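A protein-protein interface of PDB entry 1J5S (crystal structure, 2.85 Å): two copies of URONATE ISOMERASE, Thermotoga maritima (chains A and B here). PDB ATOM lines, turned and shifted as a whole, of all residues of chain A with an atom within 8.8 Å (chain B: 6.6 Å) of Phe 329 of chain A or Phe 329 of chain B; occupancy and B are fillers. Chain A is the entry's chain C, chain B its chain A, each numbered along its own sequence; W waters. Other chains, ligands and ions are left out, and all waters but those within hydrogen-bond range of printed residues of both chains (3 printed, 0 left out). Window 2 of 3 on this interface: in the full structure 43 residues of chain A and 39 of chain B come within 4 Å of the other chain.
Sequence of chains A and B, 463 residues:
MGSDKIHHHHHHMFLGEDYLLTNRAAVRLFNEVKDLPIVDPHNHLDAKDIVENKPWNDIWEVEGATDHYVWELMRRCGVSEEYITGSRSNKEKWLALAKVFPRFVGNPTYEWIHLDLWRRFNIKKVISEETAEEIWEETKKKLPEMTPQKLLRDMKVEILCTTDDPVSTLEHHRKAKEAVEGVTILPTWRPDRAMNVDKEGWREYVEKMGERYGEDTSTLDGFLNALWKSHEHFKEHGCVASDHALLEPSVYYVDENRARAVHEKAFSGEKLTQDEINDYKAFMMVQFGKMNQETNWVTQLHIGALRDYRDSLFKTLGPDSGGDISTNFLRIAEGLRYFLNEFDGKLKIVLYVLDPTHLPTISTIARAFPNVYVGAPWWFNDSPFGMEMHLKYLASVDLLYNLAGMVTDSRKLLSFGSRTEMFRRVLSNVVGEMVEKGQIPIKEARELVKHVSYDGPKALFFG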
ATOM      1  N   LEU A 247      -4.568 -15.444 -14.197  1.00  0.00           N
ATOM      2  CA  LEU A 247      -4.847 -15.786 -15.577  1.00  0.00           C
ATOM      3  C   LEU A 247      -6.053 -15.000 -16.057  1.00  0.00           C
ATOM      4  O   LEU A 247      -5.972 -14.239 -17.015  1.00  0.00           O
ATOM      5  CB  LEU A 247      -5.113 -17.278 -15.722  1.00  0.00           C
ATOM      6  CG  LEU A 247      -5.224 -17.710 -17.186  1.00  0.00           C
ATOM      7  CD1 LEU A 247      -3.872 -17.608 -17.871  1.00  0.00           C
ATOM      8  CD2 LEU A 247      -5.775 -19.117 -17.292  1.00  0.00           C
ATOM      9  N   GLU A 248      -7.169 -15.203 -15.372  1.00  0.00           N
ATOM     10  CA  GLU A 248      -8.417 -14.530 -15.674  1.00  0.00           C
ATOM     11  C   GLU A 248      -8.862 -13.779 -14.438  1.00  0.00           C
ATOM     12  O   GLU A 248      -9.572 -14.331 -13.602  1.00  0.00           O
ATOM     13  CB  GLU A 248      -9.480 -15.559 -16.044  1.00  0.00           C
ATOM     14  CG  GLU A 248      -9.808 -15.624 -17.521  1.00  0.00           C
ATOM     15  CD  GLU A 248     -11.181 -15.069 -17.824  1.00  0.00           C
ATOM     16  OE1 GLU A 248     -11.606 -14.121 -17.133  1.00  0.00           O
ATOM     17  OE2 GLU A 248     -11.842 -15.583 -18.748  1.00  0.00           O
ATOM     18  N   PRO A 249      -8.460 -12.524 -14.300  1.00  0.00           N
ATOM     19  CA  PRO A 249      -8.844 -11.774 -13.115  1.00  0.00           C
ATOM     20  C   PRO A 249     -10.338 -11.889 -12.967  1.00  0.00           C
ATOM     21  O   PRO A 249     -11.064 -11.463 -13.852  1.00  0.00           O
ATOM     22  CB  PRO A 249      -8.448 -10.340 -13.459  1.00  0.00           C
ATOM     23  CG  PRO A 249      -7.391 -10.467 -14.464  1.00  0.00           C
ATOM     24  CD  PRO A 249      -7.675 -11.709 -15.237  1.00  0.00           C
ATOM     25  N   GLY A 304      -2.592 -13.009 -17.317  1.00  0.00           N
ATOM     26  CA  GLY A 304      -2.612 -13.826 -18.515  1.00  0.00           C
ATOM     27  C   GLY A 304      -1.627 -14.943 -18.765  1.00  0.00           C
ATOM     28  O   GLY A 304      -1.546 -15.420 -19.902  1.00  0.00           O
ATOM     29  N   LEU A 306      -0.713 -18.618 -18.781  1.00  0.00           N
ATOM     30  CA  LEU A 306      -1.232 -19.968 -18.656  1.00  0.00           C
ATOM     31  C   LEU A 306       0.001 -20.786 -18.298  1.00  0.00           C
ATOM     32  O   LEU A 306       0.944 -20.856 -19.076  1.00  0.00           O
ATOM     33  CB  LEU A 306      -1.820 -20.426 -19.983  1.00  0.00           C
ATOM     34  CG  LEU A 306      -3.258 -20.948 -19.979  1.00  0.00           C
ATOM     35  CD1 LEU A 306      -3.609 -21.585 -21.341  1.00  0.00           C
ATOM     36  CD2 LEU A 306      -3.487 -21.935 -18.864  1.00  0.00           C
ATOM     37  N   SER A 326       0.872 -17.852 -23.335  1.00  0.00           N
ATOM     38  CA  SER A 326      -0.148 -16.847 -23.179  1.00  0.00           C
ATOM     39  C   SER A 326      -1.372 -17.344 -23.924  1.00  0.00           C
ATOM     40  O   SER A 326      -1.279 -18.275 -24.715  1.00  0.00           O
ATOM     41  CB  SER A 326       0.331 -15.524 -23.746  1.00  0.00           C
ATOM     42  OG  SER A 326       0.579 -15.629 -25.135  1.00  0.00           O
ATOM     43  N   THR A 327      -2.524 -16.753 -23.653  1.00  0.00           N
ATOM     44  CA  THR A 327      -3.746 -17.105 -24.349  1.00  0.00           C
ATOM     45  C   THR A 327      -4.556 -15.824 -24.525  1.00  0.00           C
ATOM     46  O   THR A 327      -4.588 -14.980 -23.637  1.00  0.00           O
ATOM     47  CB  THR A 327      -4.537 -18.163 -23.577  1.00  0.00           C
ATOM     48  OG1 THR A 327      -5.783 -18.425 -24.245  1.00  0.00           O
ATOM     49  CG2 THR A 327      -4.966 -17.681 -22.207  1.00  0.00           C
ATOM     50  N   ASN A 328      -5.190 -15.667 -25.680  1.00  0.00           N
ATOM     51  CA  ASN A 328      -5.938 -14.454 -25.986  1.00  0.00           C
ATOM     52  C   ASN A 328      -7.354 -14.486 -25.475  1.00  0.00           C
ATOM     53  O   ASN A 328      -8.104 -13.523 -25.632  1.00  0.00           O
ATOM     54  CB  ASN A 328      -6.044 -14.299 -27.488  1.00  0.00           C
ATOM     55  CG  ASN A 328      -6.656 -15.522 -28.139  1.00  0.00           C
ATOM     56  OD1 ASN A 328      -5.953 -16.492 -28.421  1.00  0.00           O
ATOM     57  ND2 ASN A 328      -7.974 -15.500 -28.356  1.00  0.00           N
ATOM     58  N   PHE A 329      -7.741 -15.598 -24.883  1.00  0.00           N
ATOM     59  CA  PHE A 329      -9.131 -15.770 -24.551  1.00  0.00           C
ATOM     60  C   PHE A 329      -9.333 -15.547 -23.054  1.00  0.00           C
ATOM     61  O   PHE A 329      -9.449 -16.489 -22.271  1.00  0.00           O
ATOM     62  CB  PHE A 329      -9.572 -17.143 -25.033  1.00  0.00           C
ATOM     63  CG  PHE A 329     -11.039 -17.308 -25.076  1.00  0.00           C
ATOM     64  CD1 PHE A 329     -11.792 -16.649 -26.020  1.00  0.00           C
ATOM     65  CD2 PHE A 329     -11.671 -18.104 -24.157  1.00  0.00           C
ATOM     66  CE1 PHE A 329     -13.152 -16.798 -26.052  1.00  0.00           C
ATOM     67  CE2 PHE A 329     -13.028 -18.261 -24.183  1.00  0.00           C
ATOM     68  CZ  PHE A 329     -13.771 -17.611 -25.130  1.00  0.00           C
ATOM     69  N   LEU A 330      -9.396 -14.271 -22.691  1.00  0.00           N
ATOM     70  CA  LEU A 330      -9.451 -13.826 -21.308  1.00  0.00           C
ATOM     71  C   LEU A 330     -10.392 -12.624 -21.122  1.00  0.00           C
ATOM     72  O   LEU A 330     -10.311 -11.636 -21.852  1.00  0.00           O
ATOM     73  CB  LEU A 330      -8.043 -13.385 -20.892  1.00  0.00           C
ATOM     74  CG  LEU A 330      -7.027 -14.295 -20.208  1.00  0.00           C
ATOM     75  CD1 LEU A 330      -7.335 -15.767 -20.324  1.00  0.00           C
ATOM     76  CD2 LEU A 330      -5.641 -13.966 -20.767  1.00  0.00           C
ATOM     77  N   ARG A 331     -11.272 -12.718 -20.132  1.00  0.00           N
ATOM     78  CA  ARG A 331     -12.195 -11.645 -19.798  1.00  0.00           C
ATOM     79  C   ARG A 331     -11.558 -10.673 -18.825  1.00  0.00           C
ATOM     80  O   ARG A 331     -11.811 -10.731 -17.631  1.00  0.00           O
ATOM     81  CB  ARG A 331     -13.438 -12.226 -19.148  1.00  0.00           C
ATOM     82  CG  ARG A 331     -14.641 -12.184 -20.031  1.00  0.00           C
ATOM     83  CD  ARG A 331     -15.968 -12.310 -19.304  1.00  0.00           C
ATOM     84  NE  ARG A 331     -15.928 -11.814 -17.933  1.00  0.00           N
ATOM     85  CZ  ARG A 331     -16.991 -11.727 -17.142  1.00  0.00           C
ATOM     86  NH1 ARG A 331     -18.183 -12.087 -17.598  1.00  0.00           N
ATOM     87  NH2 ARG A 331     -16.864 -11.273 -15.894  1.00  0.00           N
ATOM     88  N   ILE A 332     -10.762  -9.750 -19.332  1.00  0.00           N
ATOM     89  CA  ILE A 332     -10.026  -8.872 -18.446  1.00  0.00           C
ATOM     90  C   ILE A 332     -10.898  -7.829 -17.755  1.00  0.00           C
ATOM     91  O   ILE A 332     -11.007  -7.813 -16.527  1.00  0.00           O
ATOM     92  CB  ILE A 332      -8.913  -8.167 -19.203  1.00  0.00           C
ATOM     93  CG1 ILE A 332      -7.961  -9.181 -19.832  1.00  0.00           C
ATOM     94  CG2 ILE A 332      -8.170  -7.241 -18.248  1.00  0.00           C
ATOM     95  CD1 ILE A 332      -6.982  -8.536 -20.798  1.00  0.00           C
ATOM     96  N   ALA A 333     -11.504  -6.964 -18.559  1.00  0.00           N
ATOM     97  CA  ALA A 333     -12.236  -5.803 -18.076  1.00  0.00           C
ATOM     98  C   ALA A 333     -13.328  -6.102 -17.070  1.00  0.00           C
ATOM     99  O   ALA A 333     -13.412  -5.467 -16.020  1.00  0.00           O
ATOM    100  CB  ALA A 333     -12.818  -5.045 -19.247  1.00  0.00           C
ATOM    101  N   GLU A 334     -14.184  -7.054 -17.375  1.00  0.00           N
ATOM    102  CA  GLU A 334     -15.298  -7.284 -16.475  1.00  0.00           C
ATOM    103  C   GLU A 334     -14.815  -8.016 -15.224  1.00  0.00           C
ATOM    104  O   GLU A 334     -15.442  -7.937 -14.167  1.00  0.00           O
ATOM    105  CB  GLU A 334     -16.469  -7.937 -17.203  1.00  0.00           C
ATOM    106  CG  GLU A 334     -17.227  -6.908 -18.058  1.00  0.00           C
ATOM    107  CD  GLU A 334     -17.982  -5.854 -17.230  1.00  0.00           C
ATOM    108  OE1 GLU A 334     -18.090  -4.683 -17.687  1.00  0.00           O
ATOM    109  OE2 GLU A 334     -18.479  -6.190 -16.118  1.00  0.00           O
ATOM    110  N   GLY A 335     -13.663  -8.673 -15.329  1.00  0.00           N
ATOM    111  CA  GLY A 335     -13.046  -9.320 -14.181  1.00  0.00           C
ATOM    112  C   GLY A 335     -12.330  -8.380 -13.216  1.00  0.00           C
ATOM    113  O   GLY A 335     -12.217  -8.673 -12.034  1.00  0.00           O
ATOM    114  N   ASP A 355      -0.336 -11.051 -23.207  1.00  0.00           N
ATOM    115  CA  ASP A 355      -0.671 -11.078 -24.602  1.00  0.00           C
ATOM    116  C   ASP A 355      -0.837  -9.630 -25.014  1.00  0.00           C
ATOM    117  O   ASP A 355      -1.745  -8.959 -24.529  1.00  0.00           O
ATOM    118  CB  ASP A 355      -1.968 -11.820 -24.758  1.00  0.00           C
ATOM    119  CG  ASP A 355      -2.378 -11.930 -26.157  1.00  0.00           C
ATOM    120  OD1 ASP A 355      -1.821 -11.163 -26.968  1.00  0.00           O
ATOM    121  OD2 ASP A 355      -3.233 -12.750 -26.542  1.00  0.00           O
ATOM    122  N   THR A 357      -2.062  -8.294 -27.358  1.00  0.00           N
ATOM    123  CA  THR A 357      -3.415  -8.119 -27.829  1.00  0.00           C
ATOM    124  C   THR A 357      -4.358  -7.507 -26.779  1.00  0.00           C
ATOM    125  O   THR A 357      -5.442  -7.002 -27.104  1.00  0.00           O
ATOM    126  CB  THR A 357      -3.949  -9.507 -28.181  1.00  0.00           C
ATOM    127  OG1 THR A 357      -3.121 -10.107 -29.182  1.00  0.00           O
ATOM    128  CG2 THR A 357      -5.272  -9.432 -28.826  1.00  0.00           C
ATOM    129  N   HIS A 358      -3.966  -7.572 -25.514  1.00  0.00           N
ATOM    130  CA  HIS A 358      -4.816  -7.080 -24.446  1.00  0.00           C
ATOM    131  C   HIS A 358      -4.398  -5.708 -23.919  1.00  0.00           C
ATOM    132  O   HIS A 358      -5.011  -5.191 -22.979  1.00  0.00           O
ATOM    133  CB  HIS A 358      -4.833  -8.103 -23.327  1.00  0.00           C
ATOM    134  CG  HIS A 358      -5.355  -9.442 -23.752  1.00  0.00           C
ATOM    135  ND1 HIS A 358      -4.805 -10.627 -23.318  1.00  0.00           N
ATOM    136  CD2 HIS A 358      -6.379  -9.781 -24.574  1.00  0.00           C
ATOM    137  CE1 HIS A 358      -5.466 -11.639 -23.852  1.00  0.00           C
ATOM    138  NE2 HIS A 358      -6.429 -11.154 -24.614  1.00  0.00           N
ATOM    139  N   THR A 361      -7.204  -2.965 -23.713  1.00  0.00           N
ATOM    140  CA  THR A 361      -8.023  -3.079 -22.531  1.00  0.00           C
ATOM    141  C   THR A 361      -7.322  -2.376 -21.369  1.00  0.00           C
ATOM    142  O   THR A 361      -7.810  -1.369 -20.866  1.00  0.00           O
ATOM    143  CB  THR A 361      -8.271  -4.546 -22.182  1.00  0.00           C
ATOM    144  OG1 THR A 361      -8.983  -5.203 -23.250  1.00  0.00           O
ATOM    145  CG2 THR A 361      -9.211  -4.643 -21.002  1.00  0.00           C
ATOM    146  N   GLU B 248     -21.800  -5.891 -27.466  1.00  0.00           N
ATOM    147  CA  GLU B 248     -21.738  -7.224 -28.036  1.00  0.00           C
ATOM    148  C   GLU B 248     -22.886  -7.377 -29.005  1.00  0.00           C
ATOM    149  O   GLU B 248     -23.970  -7.791 -28.607  1.00  0.00           O
ATOM    150  CB  GLU B 248     -21.925  -8.251 -26.926  1.00  0.00           C
ATOM    151  CG  GLU B 248     -20.679  -9.009 -26.533  1.00  0.00           C
ATOM    152  CD  GLU B 248     -20.713 -10.431 -27.036  1.00  0.00           C
ATOM    153  OE1 GLU B 248     -21.240 -10.644 -28.146  1.00  0.00           O
ATOM    154  OE2 GLU B 248     -20.229 -11.331 -26.322  1.00  0.00           O
ATOM    155  N   THR B 327     -12.996  -3.418 -24.423  1.00  0.00           N
ATOM    156  CA  THR B 327     -12.720  -4.757 -23.929  1.00  0.00           C
ATOM    157  C   THR B 327     -12.532  -5.671 -25.130  1.00  0.00           C
ATOM    158  O   THR B 327     -13.220  -5.529 -26.126  1.00  0.00           O
ATOM    159  CB  THR B 327     -13.852  -5.266 -23.010  1.00  0.00           C
ATOM    160  OG1 THR B 327     -13.678  -6.667 -22.739  1.00  0.00           O
ATOM    161  CG2 THR B 327     -15.205  -5.196 -23.689  1.00  0.00           C
ATOM    162  N   ASN B 328     -11.583  -6.595 -25.037  1.00  0.00           N
ATOM    163  CA  ASN B 328     -11.276  -7.504 -26.139  1.00  0.00           C
ATOM    164  C   ASN B 328     -12.155  -8.720 -26.189  1.00  0.00           C
ATOM    165  O   ASN B 328     -12.039  -9.520 -27.104  1.00  0.00           O
ATOM    166  CB  ASN B 328      -9.863  -8.053 -25.974  1.00  0.00           C
ATOM    167  CG  ASN B 328      -9.686  -8.798 -24.658  1.00  0.00           C
ATOM    168  OD1 ASN B 328      -9.613  -8.178 -23.597  1.00  0.00           O
ATOM    169  ND2 ASN B 328      -9.630 -10.130 -24.717  1.00  0.00           N
ATOM    170  N   PHE B 329     -13.011  -8.881 -25.195  1.00  0.00           N
ATOM    171  CA  PHE B 329     -13.751 -10.124 -25.057  1.00  0.00           C
ATOM    172  C   PHE B 329     -15.165  -9.943 -25.583  1.00  0.00           C
ATOM    173  O   PHE B 329     -16.107  -9.770 -24.813  1.00  0.00           O
ATOM    174  CB  PHE B 329     -13.743 -10.587 -23.594  1.00  0.00           C
ATOM    175  CG  PHE B 329     -14.186 -12.012 -23.408  1.00  0.00           C
ATOM    176  CD1 PHE B 329     -13.376 -13.062 -23.812  1.00  0.00           C
ATOM    177  CD2 PHE B 329     -15.424 -12.304 -22.851  1.00  0.00           C
ATOM    178  CE1 PHE B 329     -13.787 -14.364 -23.653  1.00  0.00           C
ATOM    179  CE2 PHE B 329     -15.835 -13.610 -22.690  1.00  0.00           C
ATOM    180  CZ  PHE B 329     -15.020 -14.636 -23.092  1.00  0.00           C
ATOM    181  N   LEU B 330     -15.288 -10.004 -26.909  1.00  0.00           N
ATOM    182  CA  LEU B 330     -16.533  -9.741 -27.615  1.00  0.00           C
ATOM    183  C   LEU B 330     -16.740 -10.699 -28.786  1.00  0.00           C
ATOM    184  O   LEU B 330     -15.848 -10.882 -29.610  1.00  0.00           O
ATOM    185  CB  LEU B 330     -16.489  -8.325 -28.190  1.00  0.00           C
ATOM    186  CG  LEU B 330     -17.043  -7.102 -27.460  1.00  0.00           C
ATOM    187  CD1 LEU B 330     -17.154  -7.310 -25.970  1.00  0.00           C
ATOM    188  CD2 LEU B 330     -16.181  -5.877 -27.790  1.00  0.00           C
ATOM    189  N   ARG B 331     -17.930 -11.285 -28.863  1.00  0.00           N
ATOM    190  CA  ARG B 331     -18.314 -12.147 -29.975  1.00  0.00           C
ATOM    191  C   ARG B 331     -18.889 -11.312 -31.108  1.00  0.00           C
ATOM    192  O   ARG B 331     -20.106 -11.199 -31.253  1.00  0.00           O
ATOM    193  CB  ARG B 331     -19.395 -13.127 -29.539  1.00  0.00           C
ATOM    194  CG  ARG B 331     -18.928 -14.540 -29.386  1.00  0.00           C
ATOM    195  CD  ARG B 331     -20.053 -15.548 -29.219  1.00  0.00           C
ATOM    196  NE  ARG B 331     -21.264 -15.147 -29.931  1.00  0.00           N
ATOM    197  CZ  ARG B 331     -22.357 -15.893 -30.029  1.00  0.00           C
ATOM    198  NH1 ARG B 331     -22.390 -17.099 -29.470  1.00  0.00           N
ATOM    199  NH2 ARG B 331     -23.420 -15.432 -30.690  1.00  0.00           N
ATOM    200  N   ASP B 355     -11.811  -1.616 -30.134  1.00  0.00           N
ATOM    201  CA  ASP B 355     -10.563  -2.273 -29.843  1.00  0.00           C
ATOM    202  C   ASP B 355      -9.978  -2.613 -31.192  1.00  0.00           C
ATOM    203  O   ASP B 355     -10.563  -3.416 -31.916  1.00  0.00           O
ATOM    204  CB  ASP B 355     -10.852  -3.545 -29.069  1.00  0.00           C
ATOM    205  CG  ASP B 355      -9.608  -4.205 -28.555  1.00  0.00           C
ATOM    206  OD1 ASP B 355      -8.515  -3.971 -29.143  1.00  0.00           O
ATOM    207  OD2 ASP B 355      -9.650  -4.974 -27.562  1.00  0.00           O
ATOM    208  N   HIS B 358      -9.937  -5.950 -33.038  1.00  0.00           N
ATOM    209  CA  HIS B 358     -11.105  -6.512 -33.703  1.00  0.00           C
ATOM    210  C   HIS B 358     -11.224  -6.088 -35.177  1.00  0.00           C
ATOM    211  O   HIS B 358     -12.198  -6.445 -35.857  1.00  0.00           O
ATOM    212  CB  HIS B 358     -12.365  -6.049 -32.977  1.00  0.00           C
ATOM    213  CG  HIS B 358     -12.443  -6.477 -31.547  1.00  0.00           C
ATOM    214  ND1 HIS B 358     -12.878  -5.633 -30.548  1.00  0.00           N
ATOM    215  CD2 HIS B 358     -12.186  -7.665 -30.952  1.00  0.00           C
ATOM    216  CE1 HIS B 358     -12.866  -6.276 -29.394  1.00  0.00           C
ATOM    217  NE2 HIS B 358     -12.457  -7.512 -29.612  1.00  0.00           N
HETATM  218  O   HOH W   1      -7.354  -5.469 -25.894  1.00  0.00           O
HETATM  219  O   HOH W   2     -10.495  -3.639 -25.629  1.00  0.00           O
HETATM  220  O   HOH W   3     -11.350  -7.863 -21.869  1.00  0.00           O
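OG1 of Thr 327 of chain B sits close to N of Phe 329 of chain B (3.4 Å). OE2 of Glu 248 of chain A lies within hydrogen-bond range of N of Arg 331 of chain A, at 3.2 Å. O of Asn 328 of chain A lies within hydrogen-bond range of NE2 of His 358 of chain A, 3.1 Å away. The side-chain hydroxyl of Thr 327 of chain A sits close to the backbone NH of Phe 329 of chain A. A ring nitrogen (NE2) of His 358 of chain B lies within hydrogen-bond range of the backbone carbonyl oxygen (O) of Asn 328 of chain B (3.2 Å).
Asn 328 of chain A touches its own counterpart, Asn 328 of chain B. Phe 329 of chain B touches its own counterpart, Phe 329 of chain A. Leu 330 of chain A touches Asn 328 of chain B, but with the chains exchanged Asn 328 of chain A does not touch Leu 330 of chain B (8.1 Å). Leu 330 of chain A touches Phe 329 of chain B, but with the chains exchanged Phe 329 of chain A does not touch Leu 330 of chain B (7.2 Å). Positions printed for both chains: 248, 327, 328, 329, 330, 331, 355 and 358. Of the 10 pairs that touch across the chains among the printed residues, 2 have their exchanged pair printed and touching as well.
Phe 329 of chain A touches just one residue of chain B: Phe 329. Phe 329 of chain B touches just these residues of chain A: Phe 329, Leu 330 and Arg 331. Asn 328 of chain B touches just these residues of chain A: Asn 328, Leu 330, Ile 332, His 358 and Thr 361. Leu 330 of chain B touches none of the printed residues of chain A. Of the printed residues of chain A, Thr 327 of chain B touches Ala 333 (3.9 Å) and Thr 361 (3.8 Å). Of the printed residues of chain B, Arg 331 of chain A touches Phe 329 (2.9 Å). Of the printed residues of chain B, Leu 330 of chain A touches Asn 328 (3.3 Å) and Phe 329 (3.9 Å). Of the printed residues of chain B, Thr 361 of chain A touches Thr 327 and Asn 328. Of the printed residues of chain B, Ala 333 of chain A touches Thr 327. Glu 248 of chain B touches none of the printed residues of chain A. Leu 306 of chain A touches none of the printed residues of chain B. The nearest residue of chain B that does not touch Phe 329 of chain A is Asn 328 of chain B (5.7 Å). The nearest residue of chain A that does not touch Phe 329 of chain B is Ile 332 of chain A (5.3 Å).
The side-chain amide nitrogen of Asn 328 of chain B sits close to a ring nitrogen (NE2) of His 358 of chain A (3.4 Å). ND2 of Asn 328 of chain B is in hydrogen-bond range of O of Leu 330 of chain A (3.3 Å). The side-chain amide oxygen (OD1) of Asn 328 of chain B lies within hydrogen-bond range of the side-chain hydroxyl (OG1) of Thr 361 of chain A (3.1 Å).
Of the 8 printed residues of chain B, 3 touch a printed residue of chain A. Hydrophobic or aromatic side chains of chain B within 4 Å of the printed part of chain A: Phe 329. Hydrophobic or aromatic side chains of chain A within 4 Å of the printed part of chain B: Phe 329, Ile 332, Ala 333 and His 358. Among the printed residues, 10 pairs touch across the chains.
Water W3 lies within hydrogen-bond range of the side-chain amide oxygen of Asn 328 of chain B (2.5 Å), the side-chain hydroxyl of Thr 327 of chain B (2.8 Å), the backbone NH of Ile 332 of chain A (3.2 Å) and the backbone NH of Ala 333 of chain A (3.4 Å). Water W2 lies within hydrogen-bond range of the side-chain carboxylate of Asp 355 of chain B (2.5 Å), the backbone NH of Thr 327 of chain B (2.8 Å), the backbone NH of Asn 328 of chain B (3.2 Å) and the side-chain hydroxyl of Thr 361 of chain A (3.2 Å). Water W1 lies within hydrogen-bond range of O of Thr 357 of chain A (2.7 Å), OD2 of Asp 355 of chain B (2.9 Å) and OG1 of Thr 361 of chain A (3.1 Å).
O of Asn 328 of chain A touches ND2 of Asn 328 of chain B, 3.8 Å away. Phe 329 of chain A touches Phe 329 of chain B. Phe 329 of chain B touches Leu 330 of chain A. CG of Arg 331 of chain A touches CD2 of Phe 329 of chain B, 2.9 Å away. CD1 of Ile 332 of chain A touches OD1 of Asn 328 of chain B, at 3.9 Å. CB of Thr 327 of chain B touches CB of Ala 333 of chain A, 3.9 Å away. Thr 361 of chain A touches Thr 327 of chain B (OG1 to CA, 3.8 Å).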
